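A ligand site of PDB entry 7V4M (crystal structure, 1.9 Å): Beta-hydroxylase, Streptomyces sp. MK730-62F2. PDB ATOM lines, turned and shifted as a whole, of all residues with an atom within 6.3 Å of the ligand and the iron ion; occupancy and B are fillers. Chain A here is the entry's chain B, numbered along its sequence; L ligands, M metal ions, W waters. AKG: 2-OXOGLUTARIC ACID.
O4 of the ligand sits at hydrogen-bond distance from OH of Tyr 112 (2.5 Å).
The guanidinium group of Arg 170 lies within salt-bridge range of an oxygen (O4) of the ligand (2.6 Å).
O2 of the ligand lies within salt-bridge range of NH2 of Arg 121 (3.8 Å).
An oxygen (O2) of the ligand is in hydrogen-bond range of a ring nitrogen (NE2) of His 123, 2.8 Å away.
The backbone carbonyl oxygen (O) of Tyr 112 sits at hydrogen-bond distance from the side-chain hydroxyl (OG) of Ser 161.
The side-chain hydroxyl (OG1) of Thr 156 sits at hydrogen-bond distance from the backbone carbonyl oxygen (O) of Thr 119 (2.8 Å).
The backbone NH (N) of Leu 106 is in hydrogen-bond range of the backbone carbonyl oxygen (O) of Arg 170, 2.8 Å away.
The side-chain carboxylate of Asp 117 lies within salt-bridge range of the guanidinium group of Arg 121, 3.6 Å away.
The backbone carbonyl oxygen of Thr 156 sits close to a ring nitrogen (ND1) of His 160.
N of Val 154 lies within hydrogen-bond range of O of Arg 121 (2.9 Å).
NH1 of Arg 170 sits at hydrogen-bond distance from O of Met 104 (3.1 Å).
The backbone NH (N) of Met 104 is in hydrogen-bond range of the backbone carbonyl oxygen (O) of His 172, at 2.8 Å.
Merely in contact with the ligand: Met 104, Phe 134, Thr 156 and Ala 162.
Hydrophobic or aromatic side chains within 4 Å of the ligand: Met 104, Tyr 112, His 115, His 123, Phe 134, His 160 and Ala 162.
11 residues have an atom within 4 Å of the ligand: Met 104, Tyr 112, His 115, Asp 117, Arg 121, His 123, Phe 134, Thr 156, His 160, Ala 162 and Arg 170.
NH2 of Arg 121 touches the iron ion, 3.96 Å away.
Four residues have an atom within 4 Å of the iron ion: His 115, Asp 117, Arg 121 and His 160.
The iron ion is bound by an oxygen (O5) of the ligand (2.0 Å), the side-chain carboxylate of Asp 117 (2.1 Å), water W1 (2.1 Å), an oxygen (O1) of the ligand (2.1 Å), a ring nitrogen (NE2) of His 115 (2.3 Å) and a ring nitrogen (NE2) of His 160 (2.3 Å).
Water W1 bridges the side-chain carboxylate (OD1) of Asp 117 and the guanidinium group (NH2) of Arg 121.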
ATOM      1  N   THR A  44      -1.558   6.315  11.334  1.00  0.00           N
ATOM      2  CA  THR A  44      -1.613   6.262   9.884  1.00  0.00           C
ATOM      3  C   THR A  44      -1.957   7.649   9.398  1.00  0.00           C
ATOM      4  O   THR A  44      -3.090   8.119   9.577  1.00  0.00           O
ATOM      5  CB  THR A  44      -2.655   5.264   9.371  1.00  0.00           C
ATOM      6  OG1 THR A  44      -2.471   3.994   9.993  1.00  0.00           O
ATOM      7  CG2 THR A  44      -2.508   5.122   7.861  1.00  0.00           C
ATOM      8  N   MET A 104      -0.809   6.909   2.089  1.00  0.00           N
ATOM      9  CA  MET A 104      -0.982   6.236   3.378  1.00  0.00           C
ATOM     10  C   MET A 104       0.393   6.079   4.000  1.00  0.00           C
ATOM     11  O   MET A 104       1.259   5.394   3.440  1.00  0.00           O
ATOM     12  CB  MET A 104      -1.642   4.869   3.229  1.00  0.00           C
ATOM     13  CG  MET A 104      -2.930   4.915   2.438  1.00  0.00           C
ATOM     14  SD  MET A 104      -4.286   5.467   3.453  1.00  0.00           S
ATOM     15  CE  MET A 104      -4.747   3.888   4.163  1.00  0.00           C
ATOM     16  N   ALA A 105       0.596   6.732   5.135  1.00  0.00           N
ATOM     17  CA  ALA A 105       1.907   6.763   5.768  1.00  0.00           C
ATOM     18  C   ALA A 105       1.804   6.103   7.138  1.00  0.00           C
ATOM     19  O   ALA A 105       0.899   6.435   7.919  1.00  0.00           O
ATOM     20  CB  ALA A 105       2.394   8.198   5.893  1.00  0.00           C
ATOM     21  N   LEU A 106       2.708   5.181   7.417  1.00  0.00           N
ATOM     22  CA  LEU A 106       2.776   4.537   8.720  1.00  0.00           C
ATOM     23  C   LEU A 106       3.908   5.174   9.514  1.00  0.00           C
ATOM     24  O   LEU A 106       5.059   5.186   9.065  1.00  0.00           O
ATOM     25  CB  LEU A 106       3.012   3.027   8.581  1.00  0.00           C
ATOM     26  CG  LEU A 106       1.887   2.123   8.104  1.00  0.00           C
ATOM     27  CD1 LEU A 106       2.246   0.635   8.278  1.00  0.00           C
ATOM     28  CD2 LEU A 106       0.615   2.439   8.865  1.00  0.00           C
ATOM     29  N   TYR A 112      -1.497  -1.579  11.870  1.00  0.00           N
ATOM     30  CA  TYR A 112      -2.950  -1.522  11.755  1.00  0.00           C
ATOM     31  C   TYR A 112      -3.610  -2.635  12.550  1.00  0.00           C
ATOM     32  O   TYR A 112      -3.007  -3.679  12.834  1.00  0.00           O
ATOM     33  CB  TYR A 112      -3.396  -1.688  10.294  1.00  0.00           C
ATOM     34  CG  TYR A 112      -3.027  -0.584   9.345  1.00  0.00           C
ATOM     35  CD1 TYR A 112      -3.700   0.623   9.381  1.00  0.00           C
ATOM     36  CD2 TYR A 112      -2.029  -0.770   8.405  1.00  0.00           C
ATOM     37  CE1 TYR A 112      -3.362   1.654   8.501  1.00  0.00           C
ATOM     38  CE2 TYR A 112      -1.687   0.257   7.512  1.00  0.00           C
ATOM     39  CZ  TYR A 112      -2.373   1.451   7.572  1.00  0.00           C
ATOM     40  OH  TYR A 112      -2.048   2.453   6.682  1.00  0.00           O
ATOM     41  N   SER A 113      -4.895  -2.469  12.819  1.00  0.00           N
ATOM     42  CA  SER A 113      -5.647  -3.606  13.304  1.00  0.00           C
ATOM     43  C   SER A 113      -5.695  -4.706  12.235  1.00  0.00           C
ATOM     44  O   SER A 113      -5.436  -4.462  11.061  1.00  0.00           O
ATOM     45  CB  SER A 113      -7.071  -3.178  13.675  1.00  0.00           C
ATOM     46  OG  SER A 113      -7.741  -2.728  12.522  1.00  0.00           O
ATOM     47  N   HIS A 115      -7.837  -6.728  10.000  1.00  0.00           N
ATOM     48  CA  HIS A 115      -9.152  -6.346   9.509  1.00  0.00           C
ATOM     49  C   HIS A 115      -9.329  -6.787   8.055  1.00  0.00           C
ATOM     50  O   HIS A 115      -8.410  -7.282   7.403  1.00  0.00           O
ATOM     51  CB  HIS A 115      -9.341  -4.834   9.586  1.00  0.00           C
ATOM     52  CG  HIS A 115      -8.445  -4.084   8.668  1.00  0.00           C
ATOM     53  ND1 HIS A 115      -7.098  -3.903   8.927  1.00  0.00           N
ATOM     54  CD2 HIS A 115      -8.673  -3.507   7.460  1.00  0.00           C
ATOM     55  CE1 HIS A 115      -6.538  -3.238   7.929  1.00  0.00           C
ATOM     56  NE2 HIS A 115      -7.479  -2.989   7.027  1.00  0.00           N
ATOM     57  N   ARG A 116     -10.548  -6.602   7.553  1.00  0.00           N
ATOM     58  CA  ARG A 116     -10.889  -6.769   6.157  1.00  0.00           C
ATOM     59  C   ARG A 116     -11.408  -5.451   5.606  1.00  0.00           C
ATOM     60  O   ARG A 116     -12.060  -4.694   6.329  1.00  0.00           O
ATOM     61  CB  ARG A 116     -11.963  -7.848   5.934  1.00  0.00           C
ATOM     62  CG  ARG A 116     -11.611  -9.251   6.365  1.00  0.00           C
ATOM     63  CD  ARG A 116     -12.875 -10.135   6.281  1.00  0.00           C
ATOM     64  NE  ARG A 116     -12.637 -11.440   6.885  1.00  0.00           N
ATOM     65  CZ  ARG A 116     -12.138 -12.482   6.239  1.00  0.00           C
ATOM     66  NH1 ARG A 116     -11.808 -12.369   4.952  1.00  0.00           N
ATOM     67  NH2 ARG A 116     -11.944 -13.632   6.870  1.00  0.00           N
ATOM     68  N   ASP A 117     -11.100  -5.191   4.342  1.00  0.00           N
ATOM     69  CA  ASP A 117     -11.663  -4.053   3.641  1.00  0.00           C
ATOM     70  C   ASP A 117     -12.713  -4.548   2.655  1.00  0.00           C
ATOM     71  O   ASP A 117     -12.823  -5.740   2.368  1.00  0.00           O
ATOM     72  CB  ASP A 117     -10.587  -3.271   2.896  1.00  0.00           C
ATOM     73  CG  ASP A 117      -9.574  -2.653   3.845  1.00  0.00           C
ATOM     74  OD1 ASP A 117      -9.924  -1.763   4.644  1.00  0.00           O
ATOM     75  OD2 ASP A 117      -8.413  -3.054   3.769  1.00  0.00           O
ATOM     76  N   THR A 119     -13.003  -3.787  -0.614  1.00  0.00           N
ATOM     77  CA  THR A 119     -12.446  -4.058  -1.926  1.00  0.00           C
ATOM     78  C   THR A 119     -10.952  -4.304  -1.821  1.00  0.00           C
ATOM     79  O   THR A 119     -10.332  -3.941  -0.813  1.00  0.00           O
ATOM     80  CB  THR A 119     -12.702  -2.876  -2.885  1.00  0.00           C
ATOM     81  OG1 THR A 119     -11.870  -1.769  -2.530  1.00  0.00           O
ATOM     82  CG2 THR A 119     -14.170  -2.421  -2.809  1.00  0.00           C
ATOM     83  N   ARG A 121      -6.981  -3.545  -3.243  1.00  0.00           N
ATOM     84  CA  ARG A 121      -6.267  -2.288  -3.429  1.00  0.00           C
ATOM     85  C   ARG A 121      -4.919  -2.556  -4.049  1.00  0.00           C
ATOM     86  O   ARG A 121      -4.364  -3.651  -3.919  1.00  0.00           O
ATOM     87  CB  ARG A 121      -6.059  -1.552  -2.094  1.00  0.00           C
ATOM     88  CG  ARG A 121      -7.336  -1.175  -1.401  1.00  0.00           C
ATOM     89  CD  ARG A 121      -7.113  -0.776   0.027  1.00  0.00           C
ATOM     90  NE  ARG A 121      -8.347  -0.232   0.586  1.00  0.00           N
ATOM     91  CZ  ARG A 121      -8.439   0.355   1.772  1.00  0.00           C
ATOM     92  NH1 ARG A 121      -9.607   0.803   2.196  1.00  0.00           N
ATOM     93  NH2 ARG A 121      -7.359   0.479   2.540  1.00  0.00           N
ATOM     94  N   HIS A 123      -0.923  -1.062  -4.117  1.00  0.00           N
ATOM     95  CA  HIS A 123       0.087  -0.244  -3.446  1.00  0.00           C
ATOM     96  C   HIS A 123       1.228   0.101  -4.392  1.00  0.00           C
ATOM     97  O   HIS A 123       1.744  -0.754  -5.125  1.00  0.00           O
ATOM     98  CB  HIS A 123       0.664  -0.943  -2.217  1.00  0.00           C
ATOM     99  CG  HIS A 123      -0.320  -1.088  -1.092  1.00  0.00           C
ATOM    100  ND1 HIS A 123      -0.061  -0.619   0.169  1.00  0.00           N
ATOM    101  CD2 HIS A 123      -1.556  -1.622  -1.065  1.00  0.00           C
ATOM    102  CE1 HIS A 123      -1.114  -0.856   0.944  1.00  0.00           C
ATOM    103  NE2 HIS A 123      -2.025  -1.468   0.213  1.00  0.00           N
ATOM    104  N   PHE A 134       3.424  -6.397   4.960  1.00  0.00           N
ATOM    105  CA  PHE A 134       1.988  -6.588   4.840  1.00  0.00           C
ATOM    106  C   PHE A 134       1.734  -8.054   5.166  1.00  0.00           C
ATOM    107  O   PHE A 134       2.466  -8.922   4.686  1.00  0.00           O
ATOM    108  CB  PHE A 134       1.575  -6.194   3.422  1.00  0.00           C
ATOM    109  CG  PHE A 134       0.107  -6.174   3.190  1.00  0.00           C
ATOM    110  CD1 PHE A 134      -0.575  -7.363   2.966  1.00  0.00           C
ATOM    111  CD2 PHE A 134      -0.588  -4.974   3.135  1.00  0.00           C
ATOM    112  CE1 PHE A 134      -1.958  -7.362   2.729  1.00  0.00           C
ATOM    113  CE2 PHE A 134      -1.958  -4.962   2.899  1.00  0.00           C
ATOM    114  CZ  PHE A 134      -2.644  -6.155   2.683  1.00  0.00           C
ATOM    115  N   ILE A 145       6.384  -4.824   0.322  1.00  0.00           N
ATOM    116  CA  ILE A 145       6.119  -4.079  -0.899  1.00  0.00           C
ATOM    117  C   ILE A 145       7.280  -3.116  -1.124  1.00  0.00           C
ATOM    118  O   ILE A 145       7.366  -2.090  -0.415  1.00  0.00           O
ATOM    119  CB  ILE A 145       4.772  -3.339  -0.840  1.00  0.00           C
ATOM    120  CG1 ILE A 145       3.641  -4.376  -0.730  1.00  0.00           C
ATOM    121  CG2 ILE A 145       4.595  -2.439  -2.093  1.00  0.00           C
ATOM    122  CD1 ILE A 145       2.312  -3.802  -0.329  1.00  0.00           C
ATOM    123  N   VAL A 154      -2.977  -6.206  -3.636  1.00  0.00           N
ATOM    124  CA  VAL A 154      -3.226  -7.026  -2.454  1.00  0.00           C
ATOM    125  C   VAL A 154      -4.738  -7.149  -2.287  1.00  0.00           C
ATOM    126  O   VAL A 154      -5.446  -6.148  -2.272  1.00  0.00           O
ATOM    127  CB  VAL A 154      -2.594  -6.450  -1.170  1.00  0.00           C
ATOM    128  CG1 VAL A 154      -1.107  -6.712  -1.140  1.00  0.00           C
ATOM    129  CG2 VAL A 154      -2.849  -4.960  -1.077  1.00  0.00           C
ATOM    130  N   THR A 156      -7.202  -7.102  -0.161  1.00  0.00           N
ATOM    131  CA  THR A 156      -7.448  -6.681   1.217  1.00  0.00           C
ATOM    132  C   THR A 156      -8.852  -7.029   1.689  1.00  0.00           C
ATOM    133  O   THR A 156      -9.237  -6.631   2.796  1.00  0.00           O
ATOM    134  CB  THR A 156      -7.169  -5.183   1.348  1.00  0.00           C
ATOM    135  OG1 THR A 156      -7.769  -4.482   0.259  1.00  0.00           O
ATOM    136  CG2 THR A 156      -5.669  -4.946   1.326  1.00  0.00           C
ATOM    137  N   HIS A 160      -6.103  -9.153   7.095  1.00  0.00           N
ATOM    138  CA  HIS A 160      -4.737  -8.651   6.941  1.00  0.00           C
ATOM    139  C   HIS A 160      -4.441  -7.554   7.959  1.00  0.00           C
ATOM    140  O   HIS A 160      -5.326  -7.001   8.611  1.00  0.00           O
ATOM    141  CB  HIS A 160      -4.502  -8.105   5.511  1.00  0.00           C
ATOM    142  CG  HIS A 160      -5.288  -6.860   5.210  1.00  0.00           C
ATOM    143  ND1 HIS A 160      -6.620  -6.896   4.853  1.00  0.00           N
ATOM    144  CD2 HIS A 160      -4.935  -5.558   5.243  1.00  0.00           C
ATOM    145  CE1 HIS A 160      -7.051  -5.668   4.672  1.00  0.00           C
ATOM    146  NE2 HIS A 160      -6.046  -4.827   4.890  1.00  0.00           N
ATOM    147  N   SER A 161      -3.147  -7.261   8.078  1.00  0.00           N
ATOM    148  CA  SER A 161      -2.653  -6.049   8.708  1.00  0.00           C
ATOM    149  C   SER A 161      -1.401  -5.619   7.942  1.00  0.00           C
ATOM    150  O   SER A 161      -0.955  -6.308   7.029  1.00  0.00           O
ATOM    151  CB  SER A 161      -2.359  -6.274  10.211  1.00  0.00           C
ATOM    152  OG  SER A 161      -1.884  -5.074  10.800  1.00  0.00           O
ATOM    153  N   ALA A 162      -0.847  -4.474   8.302  1.00  0.00           N
ATOM    154  CA  ALA A 162       0.455  -4.042   7.801  1.00  0.00           C
ATOM    155  C   ALA A 162       1.162  -3.335   8.933  1.00  0.00           C
ATOM    156  O   ALA A 162       0.519  -2.789   9.829  1.00  0.00           O
ATOM    157  CB  ALA A 162       0.336  -3.114   6.581  1.00  0.00           C
ATOM    158  N   ARG A 170       6.883   5.031   6.729  1.00  0.00           N
ATOM    159  CA  ARG A 170       6.711   4.185   5.552  1.00  0.00           C
ATOM    160  C   ARG A 170       5.553   4.770   4.741  1.00  0.00           C
ATOM    161  O   ARG A 170       4.414   4.769   5.191  1.00  0.00           O
ATOM    162  CB  ARG A 170       6.446   2.736   5.970  1.00  0.00           C
ATOM    163  CG  ARG A 170       6.239   1.762   4.816  1.00  0.00           C
ATOM    164  CD  ARG A 170       4.919   1.040   4.932  1.00  0.00           C
ATOM    165  NE  ARG A 170       3.777   1.909   4.703  1.00  0.00           N
ATOM    166  CZ  ARG A 170       2.521   1.512   4.545  1.00  0.00           C
ATOM    167  NH1 ARG A 170       1.557   2.412   4.324  1.00  0.00           N
ATOM    168  NH2 ARG A 170       2.217   0.220   4.618  1.00  0.00           N
ATOM    169  N   HIS A 172       3.198   4.856   1.362  1.00  0.00           N
ATOM    170  CA  HIS A 172       2.682   4.241   0.153  1.00  0.00           C
ATOM    171  C   HIS A 172       1.640   5.160  -0.474  1.00  0.00           C
ATOM    172  O   HIS A 172       0.999   5.951   0.210  1.00  0.00           O
ATOM    173  CB  HIS A 172       1.983   2.885   0.416  1.00  0.00           C
ATOM    174  CG  HIS A 172       2.903   1.780   0.838  1.00  0.00           C
ATOM    175  ND1 HIS A 172       2.487   0.475   0.935  1.00  0.00           N
ATOM    176  CD2 HIS A 172       4.205   1.788   1.202  1.00  0.00           C
ATOM    177  CE1 HIS A 172       3.502  -0.280   1.326  1.00  0.00           C
ATOM    178  NE2 HIS A 172       4.553   0.493   1.504  1.00  0.00           N
ATOM    179  N   VAL A 174      -1.896   4.302  -2.198  1.00  0.00           N
ATOM    180  CA  VAL A 174      -2.807   3.156  -2.176  1.00  0.00           C
ATOM    181  C   VAL A 174      -4.023   3.493  -3.055  1.00  0.00           C
ATOM    182  O   VAL A 174      -4.789   4.416  -2.736  1.00  0.00           O
ATOM    183  CB  VAL A 174      -3.232   2.811  -0.741  1.00  0.00           C
ATOM    184  CG1 VAL A 174      -4.219   1.640  -0.734  1.00  0.00           C
ATOM    185  CG2 VAL A 174      -1.978   2.476   0.096  1.00  0.00           C
HETATM  186  C1  AKG L   1      -4.868  -1.806   3.021  1.00  0.00           C
HETATM  187  O1  AKG L   1      -6.084  -2.066   2.948  1.00  0.00           O
HETATM  188  O2  AKG L   1      -4.197  -1.548   1.976  1.00  0.00           O
HETATM  189  C2  AKG L   1      -4.228  -1.754   4.403  1.00  0.00           C
HETATM  190  O5  AKG L   1      -4.878  -1.982   5.438  1.00  0.00           O
HETATM  191  C3  AKG L   1      -2.748  -1.373   4.452  1.00  0.00           C
HETATM  192  C4  AKG L   1      -2.659   0.131   4.177  1.00  0.00           C
HETATM  193  C5  AKG L   1      -1.197   0.515   4.218  1.00  0.00           C
HETATM  194  O3  AKG L   1      -0.390  -0.377   3.926  1.00  0.00           O
HETATM  195  O4  AKG L   1      -0.918   1.647   4.658  1.00  0.00           O
HETATM  196 FE    FE M   1      -6.729  -2.628   4.913  1.00  0.00          FE
HETATM  197  O   HOH W   1      -7.413  -0.628   5.251  1.00  0.00           O
